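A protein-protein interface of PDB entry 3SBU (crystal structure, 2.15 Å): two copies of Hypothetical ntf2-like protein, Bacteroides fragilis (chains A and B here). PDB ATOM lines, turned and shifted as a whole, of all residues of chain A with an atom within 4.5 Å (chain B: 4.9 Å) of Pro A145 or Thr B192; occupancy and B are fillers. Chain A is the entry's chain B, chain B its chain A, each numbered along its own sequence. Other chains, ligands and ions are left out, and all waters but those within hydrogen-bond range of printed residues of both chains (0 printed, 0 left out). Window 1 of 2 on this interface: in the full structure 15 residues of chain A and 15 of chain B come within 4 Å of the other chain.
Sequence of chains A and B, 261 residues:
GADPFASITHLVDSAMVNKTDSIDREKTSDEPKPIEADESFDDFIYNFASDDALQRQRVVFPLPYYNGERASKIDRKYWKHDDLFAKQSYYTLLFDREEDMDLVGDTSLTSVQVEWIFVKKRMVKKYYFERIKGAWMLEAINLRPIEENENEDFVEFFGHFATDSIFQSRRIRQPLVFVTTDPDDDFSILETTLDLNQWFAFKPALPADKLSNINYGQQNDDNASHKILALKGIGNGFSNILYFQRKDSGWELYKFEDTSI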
ATOM      1  N   ASN A  67       2.044   2.949   2.251  1.00  0.00           N
ATOM      2  CA  ASN A  67       1.636   1.722   2.908  1.00  0.00           C
ATOM      3  C   ASN A  67       2.938   0.965   3.219  1.00  0.00           C
ATOM      4  O   ASN A  67       3.290  -0.021   2.570  1.00  0.00           O
ATOM      5  CB  ASN A  67       0.638   0.966   2.037  1.00  0.00           C
ATOM      6  CG  ASN A  67      -0.685   1.677   1.917  1.00  0.00           C
ATOM      7  OD1 ASN A  67      -1.187   1.943   0.823  1.00  0.00           O
ATOM      8  ND2 ASN A  67      -1.266   2.024   3.044  1.00  0.00           N
ATOM      9  N   GLY A  68       3.686   1.508   4.176  1.00  0.00           N
ATOM     10  CA  GLY A  68       5.007   1.013   4.542  1.00  0.00           C
ATOM     11  C   GLY A  68       5.994   1.521   3.507  1.00  0.00           C
ATOM     12  O   GLY A  68       6.184   2.737   3.387  1.00  0.00           O
ATOM     13  N   ARG A 122      -2.239  -3.688  15.507  1.00  0.00           N
ATOM     14  CA  ARG A 122      -0.804  -3.317  15.445  1.00  0.00           C
ATOM     15  C   ARG A 122      -0.487  -2.548  14.137  1.00  0.00           C
ATOM     16  O   ARG A 122       0.513  -2.776  13.459  1.00  0.00           O
ATOM     17  CB  ARG A 122       0.092  -4.545  15.615  1.00  0.00           C
ATOM     18  CG  ARG A 122      -0.124  -5.207  16.981  1.00  0.00           C
ATOM     19  CD  ARG A 122       0.837  -6.337  17.226  1.00  0.00           C
ATOM     20  NE  ARG A 122       0.524  -7.533  16.449  1.00  0.00           N
ATOM     21  CZ  ARG A 122       1.234  -8.656  16.511  1.00  0.00           C
ATOM     22  NH1 ARG A 122       2.297  -8.734  17.305  1.00  0.00           N
ATOM     23  NH2 ARG A 122       0.892  -9.710  15.778  1.00  0.00           N
ATOM     24  N   MET A 123      -1.401  -1.642  13.811  1.00  0.00           N
ATOM     25  CA  MET A 123      -1.389  -0.763  12.660  1.00  0.00           C
ATOM     26  C   MET A 123      -1.277   0.673  13.138  1.00  0.00           C
ATOM     27  O   MET A 123      -1.726   0.999  14.241  1.00  0.00           O
ATOM     28  CB  MET A 123      -2.659  -0.956  11.843  1.00  0.00           C
ATOM     29  CG  MET A 123      -2.852  -2.374  11.312  1.00  0.00           C
ATOM     30  SD  MET A 123      -1.519  -2.958  10.023  1.00  0.00           S
ATOM     31  CE  MET A 123      -1.661  -1.444   8.856  1.00  0.00           C
ATOM     32  N   LEU A 143      -0.052   4.696   6.274  1.00  0.00           N
ATOM     33  CA  LEU A 143      -0.935   3.694   6.870  1.00  0.00           C
ATOM     34  C   LEU A 143      -0.203   2.380   6.742  1.00  0.00           C
ATOM     35  O   LEU A 143      -0.047   1.881   5.640  1.00  0.00           O
ATOM     36  CB  LEU A 143      -2.326   3.652   6.207  1.00  0.00           C
ATOM     37  CG  LEU A 143      -3.292   2.634   6.824  1.00  0.00           C
ATOM     38  CD1 LEU A 143      -3.671   3.037   8.263  1.00  0.00           C
ATOM     39  CD2 LEU A 143      -4.529   2.461   5.966  1.00  0.00           C
ATOM     40  N   ARG A 144       0.306   1.852   7.841  1.00  0.00           N
ATOM     41  CA  ARG A 144       1.160   0.661   7.774  1.00  0.00           C
ATOM     42  C   ARG A 144       1.219  -0.091   9.099  1.00  0.00           C
ATOM     43  O   ARG A 144       0.787   0.463  10.127  1.00  0.00           O
ATOM     44  CB  ARG A 144       2.596   1.124   7.437  1.00  0.00           C
ATOM     45  CG  ARG A 144       3.081   2.194   8.403  1.00  0.00           C
ATOM     46  CD  ARG A 144       4.567   2.163   8.694  1.00  0.00           C
ATOM     47  NE  ARG A 144       4.921   3.376   9.431  1.00  0.00           N
ATOM     48  CZ  ARG A 144       4.809   3.526  10.749  1.00  0.00           C
ATOM     49  NH1 ARG A 144       4.416   2.509  11.510  1.00  0.00           N
ATOM     50  NH2 ARG A 144       5.135   4.679  11.320  1.00  0.00           N
ATOM     51  N   PRO A 145       1.849  -1.305   9.135  1.00  0.00           N
ATOM     52  CA  PRO A 145       2.029  -1.984  10.418  1.00  0.00           C
ATOM     53  C   PRO A 145       2.910  -1.143  11.308  1.00  0.00           C
ATOM     54  O   PRO A 145       3.693  -0.309  10.829  1.00  0.00           O
ATOM     55  CB  PRO A 145       2.705  -3.298  10.022  1.00  0.00           C
ATOM     56  CG  PRO A 145       2.311  -3.492   8.584  1.00  0.00           C
ATOM     57  CD  PRO A 145       2.444  -2.108   8.054  1.00  0.00           C
ATOM     58  N   ILE A 146       2.732  -1.311  12.611  1.00  0.00           N
ATOM     59  CA  ILE A 146       3.540  -0.631  13.619  1.00  0.00           C
ATOM     60  C   ILE A 146       5.044  -0.983  13.375  1.00  0.00           C
ATOM     61  O   ILE A 146       5.363  -2.109  12.992  1.00  0.00           O
ATOM     62  CB  ILE A 146       3.026  -1.031  15.031  1.00  0.00           C
ATOM     63  CG1 ILE A 146       3.525  -0.064  16.131  1.00  0.00           C
ATOM     64  CG2 ILE A 146       3.249  -2.526  15.364  1.00  0.00           C
ATOM     65  CD1 ILE A 146       2.623  -0.018  17.265  1.00  0.00           C
ATOM     66  N   GLU A 147       5.920   0.014  13.512  1.00  0.00           N
ATOM     67  CA  GLU A 147       7.382  -0.056  13.335  1.00  0.00           C
ATOM     68  C   GLU A 147       8.105  -0.096  14.660  1.00  0.00           C
ATOM     69  O   GLU A 147       7.483  -0.106  15.728  1.00  0.00           O
ATOM     70  CB  GLU A 147       7.881   1.234  12.645  1.00  0.00           C
ATOM     71  CG  GLU A 147       7.670   1.385  11.152  1.00  0.00           C
ATOM     72  CD  GLU A 147       8.065   2.773  10.666  1.00  0.00           C
ATOM     73  OE1 GLU A 147       8.478   3.614  11.504  1.00  0.00           O
ATOM     74  OE2 GLU A 147       7.926   3.033   9.448  1.00  0.00           O
ATOM     75  N   LEU B 176       9.425  -7.417   2.803  1.00  0.00           N
ATOM     76  CA  LEU B 176       8.499  -8.525   2.735  1.00  0.00           C
ATOM     77  C   LEU B 176       7.087  -7.998   2.398  1.00  0.00           C
ATOM     78  O   LEU B 176       6.584  -7.096   3.070  1.00  0.00           O
ATOM     79  CB  LEU B 176       8.517  -9.273   4.073  1.00  0.00           C
ATOM     80  CG  LEU B 176       7.508 -10.386   4.270  1.00  0.00           C
ATOM     81  CD1 LEU B 176       7.753 -11.537   3.276  1.00  0.00           C
ATOM     82  CD2 LEU B 176       7.585 -10.912   5.682  1.00  0.00           C
ATOM     83  N   VAL B 177       6.463  -8.527   1.329  1.00  0.00           N
ATOM     84  CA  VAL B 177       5.122  -8.085   0.950  1.00  0.00           C
ATOM     85  C   VAL B 177       4.135  -8.596   2.020  1.00  0.00           C
ATOM     86  O   VAL B 177       4.215  -9.751   2.450  1.00  0.00           O
ATOM     87  CB  VAL B 177       4.746  -8.514  -0.495  1.00  0.00           C
ATOM     88  CG1 VAL B 177       3.279  -8.219  -0.800  1.00  0.00           C
ATOM     89  CG2 VAL B 177       5.632  -7.815  -1.507  1.00  0.00           C
ATOM     90  N   PHE B 178       3.278  -7.695   2.509  1.00  0.00           N
ATOM     91  CA  PHE B 178       2.317  -8.006   3.552  1.00  0.00           C
ATOM     92  C   PHE B 178       0.944  -7.601   3.108  1.00  0.00           C
ATOM     93  O   PHE B 178       0.694  -6.444   2.753  1.00  0.00           O
ATOM     94  CB  PHE B 178       2.695  -7.332   4.882  1.00  0.00           C
ATOM     95  CG  PHE B 178       1.863  -7.664   6.086  1.00  0.00           C
ATOM     96  CD1 PHE B 178       1.566  -8.976   6.401  1.00  0.00           C
ATOM     97  CD2 PHE B 178       1.452  -6.664   6.956  1.00  0.00           C
ATOM     98  CE1 PHE B 178       0.831  -9.269   7.535  1.00  0.00           C
ATOM     99  CE2 PHE B 178       0.755  -6.964   8.109  1.00  0.00           C
ATOM    100  CZ  PHE B 178       0.447  -8.258   8.390  1.00  0.00           C
ATOM    101  N   THR B 180      -2.933  -7.409   4.351  1.00  0.00           N
ATOM    102  CA  THR B 180      -3.760  -7.521   5.539  1.00  0.00           C
ATOM    103  C   THR B 180      -5.073  -6.736   5.348  1.00  0.00           C
ATOM    104  O   THR B 180      -5.386  -6.323   4.235  1.00  0.00           O
ATOM    105  CB  THR B 180      -2.959  -7.105   6.805  1.00  0.00           C
ATOM    106  OG1 THR B 180      -3.703  -7.511   7.946  1.00  0.00           O
ATOM    107  CG2 THR B 180      -2.659  -5.615   6.866  1.00  0.00           C
ATOM    108  N   LEU B 190      -5.458  -4.259   2.444  1.00  0.00           N
ATOM    109  CA  LEU B 190      -4.345  -3.340   2.621  1.00  0.00           C
ATOM    110  C   LEU B 190      -3.052  -4.039   2.215  1.00  0.00           C
ATOM    111  O   LEU B 190      -2.664  -5.046   2.816  1.00  0.00           O
ATOM    112  CB  LEU B 190      -4.273  -2.813   4.060  1.00  0.00           C
ATOM    113  CG  LEU B 190      -2.991  -2.022   4.448  1.00  0.00           C
ATOM    114  CD1 LEU B 190      -3.028  -0.609   3.897  1.00  0.00           C
ATOM    115  CD2 LEU B 190      -2.879  -1.915   5.923  1.00  0.00           C
ATOM    116  N   GLU B 191      -2.416  -3.538   1.171  1.00  0.00           N
ATOM    117  CA  GLU B 191      -1.130  -4.098   0.790  1.00  0.00           C
ATOM    118  C   GLU B 191      -0.031  -3.189   1.277  1.00  0.00           C
ATOM    119  O   GLU B 191      -0.023  -1.992   0.990  1.00  0.00           O
ATOM    120  CB  GLU B 191      -0.999  -4.343  -0.709  1.00  0.00           C
ATOM    121  CG  GLU B 191       0.340  -5.027  -0.989  1.00  0.00           C
ATOM    122  CD  GLU B 191       0.582  -5.531  -2.399  1.00  0.00           C
ATOM    123  OE1 GLU B 191      -0.403  -5.869  -3.096  1.00  0.00           O
ATOM    124  OE2 GLU B 191       1.768  -5.631  -2.789  1.00  0.00           O
ATOM    125  N   THR B 192       0.882  -3.752   2.033  1.00  0.00           N
ATOM    126  CA  THR B 192       1.968  -2.975   2.622  1.00  0.00           C
ATOM    127  C   THR B 192       3.234  -3.834   2.591  1.00  0.00           C
ATOM    128  O   THR B 192       3.244  -4.877   1.930  1.00  0.00           O
ATOM    129  CB  THR B 192       1.547  -2.500   4.054  1.00  0.00           C
ATOM    130  OG1 THR B 192       2.520  -1.606   4.550  1.00  0.00           O
ATOM    131  CG2 THR B 192       1.412  -3.646   5.048  1.00  0.00           C
ATOM    132  N   THR B 193       4.287  -3.410   3.303  1.00  0.00           N
ATOM    133  CA  THR B 193       5.539  -4.161   3.409  1.00  0.00           C
ATOM    134  C   THR B 193       5.946  -4.252   4.859  1.00  0.00           C
ATOM    135  O   THR B 193       5.516  -3.428   5.650  1.00  0.00           O
ATOM    136  CB  THR B 193       6.653  -3.537   2.545  1.00  0.00           C
ATOM    137  OG1 THR B 193       6.900  -2.216   2.998  1.00  0.00           O
ATOM    138  CG2 THR B 193       6.339  -3.546   1.051  1.00  0.00           C
ATOM    139  N   LEU B 194       6.731  -5.281   5.219  1.00  0.00           N
ATOM    140  CA  LEU B 194       7.327  -5.467   6.552  1.00  0.00           C
ATOM    141  C   LEU B 194       8.837  -5.514   6.437  1.00  0.00           C
ATOM    142  O   LEU B 194       9.337  -6.189   5.536  1.00  0.00           O
ATOM    143  CB  LEU B 194       6.888  -6.778   7.251  1.00  0.00           C
ATOM    144  CG  LEU B 194       5.417  -7.041   7.524  1.00  0.00           C
ATOM    145  CD1 LEU B 194       5.227  -8.459   7.982  1.00  0.00           C
ATOM    146  CD2 LEU B 194       4.849  -6.103   8.594  1.00  0.00           C
ATOM    147  N   GLN B 198       9.810  -5.985  11.877  1.00  0.00           N
ATOM    148  CA  GLN B 198       8.362  -6.082  11.855  1.00  0.00           C
ATOM    149  C   GLN B 198       7.939  -7.531  11.611  1.00  0.00           C
ATOM    150  O   GLN B 198       6.948  -7.974  12.185  1.00  0.00           O
ATOM    151  CB  GLN B 198       7.755  -5.149  10.808  1.00  0.00           C
ATOM    152  CG  GLN B 198       7.890  -3.666  11.145  1.00  0.00           C
ATOM    153  CD  GLN B 198       7.481  -2.821   9.958  1.00  0.00           C
ATOM    154  OE1 GLN B 198       7.964  -2.985   8.831  1.00  0.00           O
ATOM    155  NE2 GLN B 198       6.489  -1.997  10.139  1.00  0.00           N
ATOM    156  N   PHE B 202       5.297  -9.786  13.895  1.00  0.00           N
ATOM    157  CA  PHE B 202       4.029 -10.203  13.285  1.00  0.00           C
ATOM    158  C   PHE B 202       3.972 -11.673  12.903  1.00  0.00           C
ATOM    159  O   PHE B 202       2.884 -12.183  12.632  1.00  0.00           O
ATOM    160  CB  PHE B 202       3.797  -9.373  12.011  1.00  0.00           C
ATOM    161  CG  PHE B 202       3.256  -7.987  12.252  1.00  0.00           C
ATOM    162  CD1 PHE B 202       1.884  -7.766  12.339  1.00  0.00           C
ATOM    163  CD2 PHE B 202       4.117  -6.910  12.442  1.00  0.00           C
ATOM    164  CE1 PHE B 202       1.384  -6.492  12.605  1.00  0.00           C
ATOM    165  CE2 PHE B 202       3.619  -5.630  12.682  1.00  0.00           C
ATOM    166  CZ  PHE B 202       2.255  -5.429  12.767  1.00  0.00           C
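Among the printed residues, pairs that only touch across the chains: Asn A67 with Glu B191 (3.2 Å), Met A123 with Leu B190 (3.2 Å), Arg A122 with Phe B202 (3.2 Å), Asn A67 with Leu B190 (3.3 Å), Pro A145 with Phe B202 (3.5 Å), Pro A145 with Thr B192 (3.5 Å), Asn A67 with Thr B193 (3.6 Å), Pro A145 with Leu B194 (3.6 Å), Pro A145 with Phe B178 (3.7 Å), Glu A147 with Gln B198 (3.7 Å), Gly A68 with Thr B193 (3.9 Å), Ile A146 with Phe B202 (3.9 Å), Arg A144 with Thr B192 (3.97 Å) and Leu A143 with Leu B190 (3.99 Å).
No position is printed for both chains. Of the 18 pairs that touch across the chains among the printed residues, none has its exchanged pair printed and touching as well.
Of the 11 printed residues of chain B, 8 touch a printed residue of chain A. Printed residues of chain B that touch a printed residue of chain A: Phe B178, Leu B190, Glu B191, Thr B192, Thr B193, Leu B194, Gln B198 and Phe B202. Of the 9 printed residues of chain A, 9 touch a printed residue of chain B. Printed residues of chain A that touch a printed residue of chain B: Asn A67, Gly A68, Arg A122, Met A123, Leu A143, Arg A144, Pro A145, Ile A146 and Glu A147.
O of Phe B178 lies within hydrogen-bond range of N of Thr B192 (2.8 Å). The backbone carbonyl oxygen (O) of Leu A143 lies within hydrogen-bond range of the side-chain amide nitrogen (ND2) of Asn A67 (2.9 Å). O of Thr B180 lies within hydrogen-bond range of N of Leu B190, at 2.7 Å. O of Leu B176 sits at hydrogen-bond distance from N of Leu B194 (2.8 Å). The backbone carbonyl oxygen (O) of Arg A122 sits at hydrogen-bond distance from the backbone NH (N) of Ile A146, 2.8 Å away. The side-chain carboxylate of Glu A147 is in salt-bridge range of the guanidinium group of Arg A144, 3.0 Å away.
OG1 of Thr B192 sits at hydrogen-bond distance from N of Gly A68, at 3.3 Å. NE2 of Gln B198 lies within hydrogen-bond range of O of Pro A145 (3.3 Å). The backbone carbonyl oxygen (O) of Asn A67 is in hydrogen-bond range of the side-chain hydroxyl (OG1) of Thr B192 (2.7 Å). The side-chain amide nitrogen of Gln B198 is in hydrogen-bond range of the backbone carbonyl oxygen of Ile A146 (3.1 Å).
Of the printed residues of chain B, Arg A122 touches Phe B202 (3.2 Å). Printed residues of chain B within 4 Å of Met A123: Leu B190. Printed residues of chain B within 4 Å of Pro A145: Phe B178 (3.7 Å), Thr B192 (3.5 Å), Leu B194 (3.6 Å), Gln B198 (3.3 Å) and Phe B202 (3.5 Å). Printed residues of chain B within 4 Å of Glu A147: Gln B198. Printed residues of chain A within 4 Å of Glu B191: Asn A67. Thr B192 touches just these residues of chain A: Asn A67 (2.7 Å), Gly A68 (3.3 Å), Arg A144 (3.97 Å) and Pro A145 (3.5 Å). Of the printed residues of chain A, Gln B198 touches Pro A145, Ile A146 and Glu A147.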
